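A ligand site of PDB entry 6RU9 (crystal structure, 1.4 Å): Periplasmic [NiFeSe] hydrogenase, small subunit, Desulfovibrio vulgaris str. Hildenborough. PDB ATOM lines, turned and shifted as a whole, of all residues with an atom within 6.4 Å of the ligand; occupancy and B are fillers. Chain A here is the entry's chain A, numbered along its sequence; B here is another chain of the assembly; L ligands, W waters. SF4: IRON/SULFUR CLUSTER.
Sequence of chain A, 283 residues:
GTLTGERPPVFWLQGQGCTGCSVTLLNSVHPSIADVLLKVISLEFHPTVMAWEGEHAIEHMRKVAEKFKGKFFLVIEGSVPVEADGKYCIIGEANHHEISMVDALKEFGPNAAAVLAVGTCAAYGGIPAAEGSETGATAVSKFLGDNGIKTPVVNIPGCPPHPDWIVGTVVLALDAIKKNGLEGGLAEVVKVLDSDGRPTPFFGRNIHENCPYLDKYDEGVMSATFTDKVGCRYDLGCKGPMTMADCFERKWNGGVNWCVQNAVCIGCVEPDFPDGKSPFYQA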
ATOM      1  N   GLN A  16     -15.997   6.316 -19.077  1.00  0.00           N
ATOM      2  CA  GLN A  16     -15.639   4.912 -19.150  1.00  0.00           C
ATOM      3  C   GLN A  16     -14.966   4.533 -17.842  1.00  0.00           C
ATOM      4  O   GLN A  16     -13.764   4.300 -17.773  1.00  0.00           O
ATOM      5  CB  GLN A  16     -14.695   4.657 -20.330  1.00  0.00           C
ATOM      6  CG  GLN A  16     -15.324   4.754 -21.648  1.00  0.00           C
ATOM      7  CD  GLN A  16     -14.303   4.674 -22.772  1.00  0.00           C
ATOM      8  OE1 GLN A  16     -13.406   5.493 -22.833  1.00  0.00           O
ATOM      9  NE2 GLN A  16     -14.440   3.676 -23.643  1.00  0.00           N
ATOM     10  N   GLY A  17     -15.777   4.547 -16.775  1.00  0.00           N
ATOM     11  CA  GLY A  17     -15.303   4.206 -15.450  1.00  0.00           C
ATOM     12  C   GLY A  17     -15.928   2.892 -14.996  1.00  0.00           C
ATOM     13  O   GLY A  17     -16.855   2.359 -15.610  1.00  0.00           O
ATOM     14  N   CYS A  18     -15.381   2.351 -13.909  1.00  0.00           N
ATOM     15  CA  CYS A  18     -15.911   1.137 -13.336  1.00  0.00           C
ATOM     16  C   CYS A  18     -16.661   1.391 -12.025  1.00  0.00           C
ATOM     17  O   CYS A  18     -17.085   0.424 -11.387  1.00  0.00           O
ATOM     18  CB  CYS A  18     -14.785   0.114 -13.093  1.00  0.00           C
ATOM     19  SG  CYS A  18     -13.771   0.443 -11.626  1.00  0.00           S
ATOM     20  N   THR A  19     -16.826   2.657 -11.611  1.00  0.00           N
ATOM     21  CA  THR A  19     -17.449   3.084 -10.352  1.00  0.00           C
ATOM     22  C   THR A  19     -16.509   2.835  -9.182  1.00  0.00           C
ATOM     23  O   THR A  19     -16.831   3.203  -8.037  1.00  0.00           O
ATOM     24  CB  THR A  19     -18.861   2.512 -10.205  1.00  0.00           C
ATOM     25  OG1 THR A  19     -19.588   2.862 -11.409  1.00  0.00           O
ATOM     26  CG2 THR A  19     -19.591   3.108  -9.045  1.00  0.00           C
ATOM     27  N   GLY A  20     -15.322   2.297  -9.420  1.00  0.00           N
ATOM     28  CA  GLY A  20     -14.359   2.115  -8.354  1.00  0.00           C
ATOM     29  C   GLY A  20     -13.884   3.386  -7.705  1.00  0.00           C
ATOM     30  O   GLY A  20     -13.550   3.376  -6.515  1.00  0.00           O
ATOM     31  N   CYS A  21     -13.854   4.490  -8.456  1.00  0.00           N
ATOM     32  CA  CYS A  21     -13.426   5.774  -7.888  1.00  0.00           C
ATOM     33  C   CYS A  21     -14.508   6.361  -6.987  1.00  0.00           C
ATOM     34  O   CYS A  21     -14.202   7.023  -5.992  1.00  0.00           O
ATOM     35  CB  CYS A  21     -12.953   6.711  -9.011  1.00  0.00           C
ATOM     36  SG  CYS A  21     -11.408   6.154  -9.850  1.00  0.00           S
ATOM     37  N   SER A  22     -15.785   6.091  -7.296  1.00  0.00           N
ATOM     38  CA  SER A  22     -16.869   6.412  -6.385  1.00  0.00           C
ATOM     39  C   SER A  22     -16.823   5.535  -5.133  1.00  0.00           C
ATOM     40  O   SER A  22     -16.978   6.032  -4.012  1.00  0.00           O
ATOM     41  CB  SER A  22     -18.229   6.302  -7.075  1.00  0.00           C
ATOM     42  OG  SER A  22     -18.377   7.355  -8.017  1.00  0.00           O
ATOM     43  N   GLU A  77     -14.839  10.723 -13.583  1.00  0.00           N
ATOM     44  CA  GLU A  77     -14.403   9.357 -13.306  1.00  0.00           C
ATOM     45  C   GLU A  77     -14.492   8.619 -14.638  1.00  0.00           C
ATOM     46  O   GLU A  77     -15.546   8.632 -15.276  1.00  0.00           O
ATOM     47  CB  GLU A  77     -15.335   8.708 -12.268  1.00  0.00           C
ATOM     48  CG  GLU A  77     -15.197   7.199 -12.069  1.00  0.00           C
ATOM     49  CD  GLU A  77     -16.031   6.653 -10.884  1.00  0.00           C
ATOM     50  OE1 GLU A  77     -16.999   7.312 -10.438  1.00  0.00           O
ATOM     51  OE2 GLU A  77     -15.726   5.541 -10.366  1.00  0.00           O
ATOM     52  N   GLY A  78     -13.415   7.969 -15.057  1.00  0.00           N
ATOM     53  CA  GLY A  78     -13.387   7.246 -16.306  1.00  0.00           C
ATOM     54  C   GLY A  78     -12.824   8.089 -17.430  1.00  0.00           C
ATOM     55  O   GLY A  78     -12.694   9.315 -17.332  1.00  0.00           O
ATOM     56  N   SER A  79     -12.399   7.409 -18.503  1.00  0.00           N
ATOM     57  CA  SER A  79     -11.880   8.053 -19.698  1.00  0.00           C
ATOM     58  C   SER A  79     -13.012   8.548 -20.605  1.00  0.00           C
ATOM     59  O   SER A  79     -14.193   8.205 -20.416  1.00  0.00           O
ATOM     60  CB  SER A  79     -10.948   7.098 -20.435  1.00  0.00           C
ATOM     61  OG  SER A  79     -11.556   5.880 -20.734  1.00  0.00           O
ATOM     62  N   VAL A 118     -10.428  12.154 -11.566  1.00  0.00           N
ATOM     63  CA  VAL A 118     -10.257  11.183 -10.478  1.00  0.00           C
ATOM     64  C   VAL A 118     -10.052   9.807 -11.087  1.00  0.00           C
ATOM     65  O   VAL A 118     -10.864   9.349 -11.898  1.00  0.00           O
ATOM     66  CB  VAL A 118     -11.465  11.219  -9.524  1.00  0.00           C
ATOM     67  CG1 VAL A 118     -11.386  10.075  -8.547  1.00  0.00           C
ATOM     68  CG2 VAL A 118     -11.497  12.566  -8.771  1.00  0.00           C
ATOM     69  N   GLY A 119      -9.000   9.146 -10.660  1.00  0.00           N
ATOM     70  CA  GLY A 119      -8.654   7.829 -11.166  1.00  0.00           C
ATOM     71  C   GLY A 119      -7.737   7.882 -12.377  1.00  0.00           C
ATOM     72  O   GLY A 119      -7.706   8.860 -13.156  1.00  0.00           O
ATOM     73  N   THR A 120      -6.966   6.808 -12.547  1.00  0.00           N
ATOM     74  CA  THR A 120      -6.034   6.735 -13.681  1.00  0.00           C
ATOM     75  C   THR A 120      -6.719   6.788 -15.036  1.00  0.00           C
ATOM     76  O   THR A 120      -6.138   7.330 -15.984  1.00  0.00           O
ATOM     77  CB  THR A 120      -5.130   5.515 -13.485  1.00  0.00           C
ATOM     78  OG1 THR A 120      -4.400   5.773 -12.279  1.00  0.00           O
ATOM     79  CG2 THR A 120      -4.211   5.266 -14.711  1.00  0.00           C
ATOM     80  N   CYS A 121      -7.939   6.260 -15.165  1.00  0.00           N
ATOM     81  CA  CYS A 121      -8.622   6.340 -16.459  1.00  0.00           C
ATOM     82  C   CYS A 121      -8.829   7.795 -16.865  1.00  0.00           C
ATOM     83  O   CYS A 121      -8.464   8.181 -17.974  1.00  0.00           O
ATOM     84  CB  CYS A 121      -9.993   5.661 -16.370  1.00  0.00           C
ATOM     85  SG  CYS A 121      -9.997   3.903 -16.086  1.00  0.00           S
ATOM     86  N   ALA A 122      -9.442   8.592 -15.981  1.00  0.00           N
ATOM     87  CA  ALA A 122      -9.672  10.005 -16.271  1.00  0.00           C
ATOM     88  C   ALA A 122      -8.361  10.752 -16.389  1.00  0.00           C
ATOM     89  O   ALA A 122      -8.200  11.614 -17.266  1.00  0.00           O
ATOM     90  CB  ALA A 122     -10.545  10.591 -15.169  1.00  0.00           C
ATOM     91  N   ILE A 127      -6.858   1.698 -18.170  1.00  0.00           N
ATOM     92  CA  ILE A 127      -7.183   0.429 -18.833  1.00  0.00           C
ATOM     93  C   ILE A 127      -8.010   0.626 -20.085  1.00  0.00           C
ATOM     94  O   ILE A 127      -7.713  -0.013 -21.101  1.00  0.00           O
ATOM     95  CB  ILE A 127      -7.758  -0.576 -17.832  1.00  0.00           C
ATOM     96  CG1 ILE A 127      -6.665  -0.986 -16.851  1.00  0.00           C
ATOM     97  CG2 ILE A 127      -8.277  -1.805 -18.573  1.00  0.00           C
ATOM     98  CD1 ILE A 127      -7.100  -1.868 -15.732  1.00  0.00           C
ATOM     99  N   PRO A 128      -9.027   1.507 -20.132  1.00  0.00           N
ATOM    100  CA  PRO A 128      -9.784   1.645 -21.394  1.00  0.00           C
ATOM    101  C   PRO A 128      -8.936   2.126 -22.573  1.00  0.00           C
ATOM    102  O   PRO A 128      -9.347   1.936 -23.745  1.00  0.00           O
ATOM    103  CB  PRO A 128     -10.863   2.684 -21.020  1.00  0.00           C
ATOM    104  CG  PRO A 128     -11.060   2.495 -19.541  1.00  0.00           C
ATOM    105  CD  PRO A 128      -9.674   2.218 -19.011  1.00  0.00           C
ATOM    106  N   GLY A 158      -4.668   6.690  -9.596  1.00  0.00           N
ATOM    107  CA  GLY A 158      -4.842   5.500  -8.816  1.00  0.00           C
ATOM    108  C   GLY A 158      -5.963   4.704  -9.416  1.00  0.00           C
ATOM    109  O   GLY A 158      -6.858   5.270 -10.076  1.00  0.00           O
ATOM    110  N   CYS A 159      -5.942   3.394  -9.260  1.00  0.00           N
ATOM    111  CA  CYS A 159      -6.931   2.510  -9.861  1.00  0.00           C
ATOM    112  C   CYS A 159      -7.342   1.481  -8.815  1.00  0.00           C
ATOM    113  O   CYS A 159      -6.926   0.337  -8.870  1.00  0.00           O
ATOM    114  CB  CYS A 159      -6.363   1.827 -11.111  1.00  0.00           C
ATOM    115  SG  CYS A 159      -7.619   1.011 -12.136  1.00  0.00           S
ATOM    116  N   PRO A 160      -8.110   1.895  -7.801  1.00  0.00           N
ATOM    117  CA  PRO A 160      -8.600   3.262  -7.633  1.00  0.00           C
ATOM    118  C   PRO A 160      -7.640   4.100  -6.800  1.00  0.00           C
ATOM    119  O   PRO A 160      -6.728   3.572  -6.175  1.00  0.00           O
ATOM    120  CB  PRO A 160      -9.873   3.069  -6.824  1.00  0.00           C
ATOM    121  CG  PRO A 160      -9.509   1.905  -5.905  1.00  0.00           C
ATOM    122  CD  PRO A 160      -8.583   1.021  -6.700  1.00  0.00           C
ATOM    123  N   PRO A 161      -7.889   5.413  -6.752  1.00  0.00           N
ATOM    124  CA  PRO A 161      -7.191   6.264  -5.791  1.00  0.00           C
ATOM    125  C   PRO A 161      -7.570   5.844  -4.375  1.00  0.00           C
ATOM    126  O   PRO A 161      -8.620   5.236  -4.152  1.00  0.00           O
ATOM    127  CB  PRO A 161      -7.715   7.676  -6.098  1.00  0.00           C
ATOM    128  CG  PRO A 161      -8.350   7.578  -7.464  1.00  0.00           C
ATOM    129  CD  PRO A 161      -8.882   6.155  -7.563  1.00  0.00           C
ATOM    130  N   PHE A 273       0.122   3.201 -16.661  1.00  0.00           N
ATOM    131  CA  PHE A 273      -0.622   2.036 -16.185  1.00  0.00           C
ATOM    132  C   PHE A 273      -1.790   1.770 -17.113  1.00  0.00           C
ATOM    133  O   PHE A 273      -2.565   2.685 -17.414  1.00  0.00           O
ATOM    134  CB  PHE A 273      -1.132   2.299 -14.787  1.00  0.00           C
ATOM    135  CG  PHE A 273      -1.967   1.203 -14.235  1.00  0.00           C
ATOM    136  CD1 PHE A 273      -1.384   0.117 -13.601  1.00  0.00           C
ATOM    137  CD2 PHE A 273      -3.340   1.253 -14.316  1.00  0.00           C
ATOM    138  CE1 PHE A 273      -2.144  -0.908 -13.075  1.00  0.00           C
ATOM    139  CE2 PHE A 273      -4.135   0.239 -13.794  1.00  0.00           C
ATOM    140  CZ  PHE A 273      -3.535  -0.847 -13.162  1.00  0.00           C
ATOM    141  N   ARG B  50     -16.200  -0.563 -23.094  1.00  0.00           N
ATOM    142  CA  ARG B  50     -14.749  -0.502 -22.972  1.00  0.00           C
ATOM    143  C   ARG B  50     -14.031  -1.597 -23.763  1.00  0.00           C
ATOM    144  O   ARG B  50     -12.976  -1.330 -24.321  1.00  0.00           O
ATOM    145  CB  ARG B  50     -14.322  -0.537 -21.496  1.00  0.00           C
ATOM    146  CG  ARG B  50     -14.572   0.817 -20.799  1.00  0.00           C
ATOM    147  CD  ARG B  50     -14.612   0.775 -19.244  1.00  0.00           C
ATOM    148  NE  ARG B  50     -15.585  -0.188 -18.811  1.00  0.00           N
ATOM    149  CZ  ARG B  50     -15.567  -0.796 -17.643  1.00  0.00           C
ATOM    150  NH1 ARG B  50     -14.633  -0.471 -16.747  1.00  0.00           N
ATOM    151  NH2 ARG B  50     -16.458  -1.723 -17.405  1.00  0.00           N
ATOM    152  N   PHE B  52     -13.039  -5.054 -22.666  1.00  0.00           N
ATOM    153  CA  PHE B  52     -12.017  -5.826 -21.950  1.00  0.00           C
ATOM    154  C   PHE B  52     -11.611  -7.085 -22.715  1.00  0.00           C
ATOM    155  O   PHE B  52     -10.446  -7.524 -22.632  1.00  0.00           O
ATOM    156  CB  PHE B  52     -12.526  -6.194 -20.536  1.00  0.00           C
ATOM    157  CG  PHE B  52     -12.381  -5.074 -19.572  1.00  0.00           C
ATOM    158  CD1 PHE B  52     -13.231  -3.988 -19.623  1.00  0.00           C
ATOM    159  CD2 PHE B  52     -11.365  -5.065 -18.629  1.00  0.00           C
ATOM    160  CE1 PHE B  52     -13.086  -2.908 -18.763  1.00  0.00           C
ATOM    161  CE2 PHE B  52     -11.224  -4.000 -17.752  1.00  0.00           C
ATOM    162  CZ  PHE B  52     -12.084  -2.908 -17.831  1.00  0.00           C
ATOM    163  N   ARG B  70     -11.082  -4.393 -13.127  1.00  0.00           N
ATOM    164  CA  ARG B  70     -11.468  -3.065 -13.551  1.00  0.00           C
ATOM    165  C   ARG B  70     -12.700  -3.051 -14.409  1.00  0.00           C
ATOM    166  O   ARG B  70     -13.118  -1.975 -14.835  1.00  0.00           O
ATOM    167  CB  ARG B  70     -10.303  -2.334 -14.207  1.00  0.00           C
ATOM    168  CG  ARG B  70      -9.317  -1.777 -13.172  1.00  0.00           C
ATOM    169  CD  ARG B  70      -8.385  -2.847 -12.545  1.00  0.00           C
ATOM    170  NE  ARG B  70      -7.528  -2.226 -11.543  1.00  0.00           N
ATOM    171  CZ  ARG B  70      -6.769  -2.895 -10.672  1.00  0.00           C
ATOM    172  NH1 ARG B  70      -6.722  -4.211 -10.699  1.00  0.00           N
ATOM    173  NH2 ARG B  70      -6.079  -2.214  -9.762  1.00  0.00           N
ATOM    174  N   ILE B  71     -13.254  -4.215 -14.729  1.00  0.00           N
ATOM    175  CA  ILE B  71     -14.610  -4.219 -15.274  1.00  0.00           C
ATOM    176  C   ILE B  71     -15.541  -3.452 -14.335  1.00  0.00           C
ATOM    177  O   ILE B  71     -16.428  -2.726 -14.778  1.00  0.00           O
ATOM    178  CB  ILE B  71     -15.088  -5.653 -15.494  1.00  0.00           C
ATOM    179  CG1 ILE B  71     -14.333  -6.280 -16.654  1.00  0.00           C
ATOM    180  CG2 ILE B  71     -16.579  -5.721 -15.739  1.00  0.00           C
ATOM    181  CD1 ILE B  71     -14.542  -7.732 -16.830  1.00  0.00           C
ATOM    182  N   CYS B  72     -15.358  -3.628 -13.018  1.00  0.00           N
ATOM    183  CA  CYS B  72     -16.321  -3.087 -12.070  1.00  0.00           C
ATOM    184  C   CYS B  72     -15.723  -2.928 -10.699  1.00  0.00           C
ATOM    185  O   CYS B  72     -15.189  -3.876 -10.131  1.00  0.00           O
ATOM    186  CB  CYS B  72     -17.538  -4.015 -12.024  1.00  0.00           C
ATOM    187  SG  CYS B  72     -18.775  -3.369 -10.893  1.00  0.00           S
ATOM    188  N   GLY B  73     -15.837  -1.723 -10.147  1.00  0.00           N
ATOM    189  CA  GLY B  73     -15.348  -1.434  -8.819  1.00  0.00           C
ATOM    190  C   GLY B  73     -16.289  -1.735  -7.676  1.00  0.00           C
ATOM    191  O   GLY B  73     -15.918  -1.589  -6.509  1.00  0.00           O
ATOM    192  N   PRO B 181     -11.564  -1.028  -3.426  1.00  0.00           N
ATOM    193  CA  PRO B 181     -11.674  -1.893  -4.604  1.00  0.00           C
ATOM    194  C   PRO B 181     -10.344  -2.375  -5.178  1.00  0.00           C
ATOM    195  O   PRO B 181      -9.285  -1.794  -4.933  1.00  0.00           O
ATOM    196  CB  PRO B 181     -12.371  -1.001  -5.639  1.00  0.00           C
ATOM    197  CG  PRO B 181     -13.131   0.012  -4.832  1.00  0.00           C
ATOM    198  CD  PRO B 181     -12.244   0.266  -3.626  1.00  0.00           C
ATOM    199  N   HIS B 182     -10.435  -3.501  -5.919  1.00  0.00           N
ATOM    200  CA  HIS B 182      -9.364  -4.058  -6.729  1.00  0.00           C
ATOM    201  C   HIS B 182      -8.327  -4.727  -5.875  1.00  0.00           C
ATOM    202  O   HIS B 182      -7.237  -4.198  -5.635  1.00  0.00           O
ATOM    203  CB  HIS B 182      -8.816  -3.023  -7.708  1.00  0.00           C
ATOM    204  CG  HIS B 182      -9.884  -2.466  -8.601  1.00  0.00           C
ATOM    205  ND1 HIS B 182     -11.024  -3.173  -8.908  1.00  0.00           N
ATOM    206  CD2 HIS B 182      -9.977  -1.280  -9.251  1.00  0.00           C
ATOM    207  CE1 HIS B 182     -11.796  -2.437  -9.684  1.00  0.00           C
ATOM    208  NE2 HIS B 182     -11.185  -1.284  -9.909  1.00  0.00           N
HETATM  209 FE1  SF4 L   1     -12.242   2.062 -12.220  1.00  0.00          FE
HETATM  210 FE2  SF4 L   1     -10.823   3.638 -13.879  1.00  0.00          FE
HETATM  211 FE3  SF4 L   1      -9.523   2.258 -11.973  1.00  0.00          FE
HETATM  212 FE4  SF4 L   1     -11.194   4.335 -11.199  1.00  0.00          FE
HETATM  213  S1  SF4 L   1      -9.229   4.490 -12.445  1.00  0.00           S
HETATM  214  S2  SF4 L   1     -10.996   2.145 -10.218  1.00  0.00           S
HETATM  215  S3  SF4 L   1     -12.814   4.231 -12.845  1.00  0.00           S
HETATM  216  S4  SF4 L   1     -10.743   1.324 -13.794  1.00  0.00           S
HETATM  217  O   HOH W   1     -12.726   1.699 -16.645  1.00  0.00           O
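Water W1 lies within hydrogen-bond range of the guanidinium group of Arg 50 of chain B (2.9 Å), the backbone carbonyl oxygen of Gln 16 (3.0 Å) and a sulfur (S4) of the ligand (3.5 Å).
The side-chain carboxylate (OE2) of Glu 77 sits at hydrogen-bond distance from the backbone NH (N) of Cys 21.
NH2 of Arg 70 of chain B lies within hydrogen-bond range of O of Cys 159 (2.8 Å).
The side-chain sulfur (SG) of Cys 18 sits close to a ring nitrogen (NE2) of His 182 of chain B (3.6 Å).
The backbone carbonyl oxygen (O) of Cys 18 lies within hydrogen-bond range of the backbone NH (N) of Gly 73 of chain B (2.8 Å).
The backbone NH of Gly 158 lies within hydrogen-bond range of the side-chain hydroxyl of Thr 120 (2.8 Å).
The backbone NH (N) of Gly 20 is in hydrogen-bond range of the side-chain carboxylate (OE2) of Glu 77, 3.4 Å away.
The side-chain carboxylate of Glu 77 lies close to the backbone NH of Thr 19, at 3.3 Å.
OE1 of Glu 77 lies within hydrogen-bond range of OG of Ser 22, 2.8 Å away.
The backbone carbonyl oxygen (O) of Gly 158 lies close to a sulfur (S1) of the ligand (3.4 Å).
A sulfur (S2) of the ligand sits close to the backbone nitrogen of Pro 160.
Gly 17 touches the ligand (CA to S3, 3.6 Å).
Gly 20 touches the ligand (CA to S2, 3.8 Å).
Glu 77 touches the ligand.
CA of Gly 119 touches S1 of the ligand (3.6 Å).
Arg 70 of chain B touches the ligand (CG to S4, 3.5 Å).
Hydrophobic or aromatic side chains within 4 Å of the ligand: Pro 160 and His 182 of chain B.
13 residues have an atom within 4 Å of the ligand: Gly 17, Cys 18, Gly 20, Cys 21, Glu 77, Gly 119, Thr 120, Cys 121, Gly 158, Cys 159, Pro 160, Arg 70 of chain B and His 182 of chain B.
The nearest printed residue that does not touch the ligand is Gly 78 (4.4 Å).
FE4 of the ligand is bound by SG of Cys 21.
An iron atom (FE3) of the ligand is bound by the side-chain sulfur of Cys 159, 2.3 Å away.
The backbone NH (N) of Cys 18 lies close to a sulfur (S3) of the ligand (3.4 Å).
The side-chain sulfur (SG) of Cys 18 is bound to an iron atom (FE1) of the ligand.
N of Cys 121 lies close to S1 of the ligand, at 3.5 Å.
The side-chain sulfur (SG) of Cys 121 binds an iron atom (FE2) of the ligand (2.4 Å).
N of Thr 120 lies close to S1 of the ligand.
NE2 of His 182 of chain B lies close to S2 of the ligand (3.4 Å).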
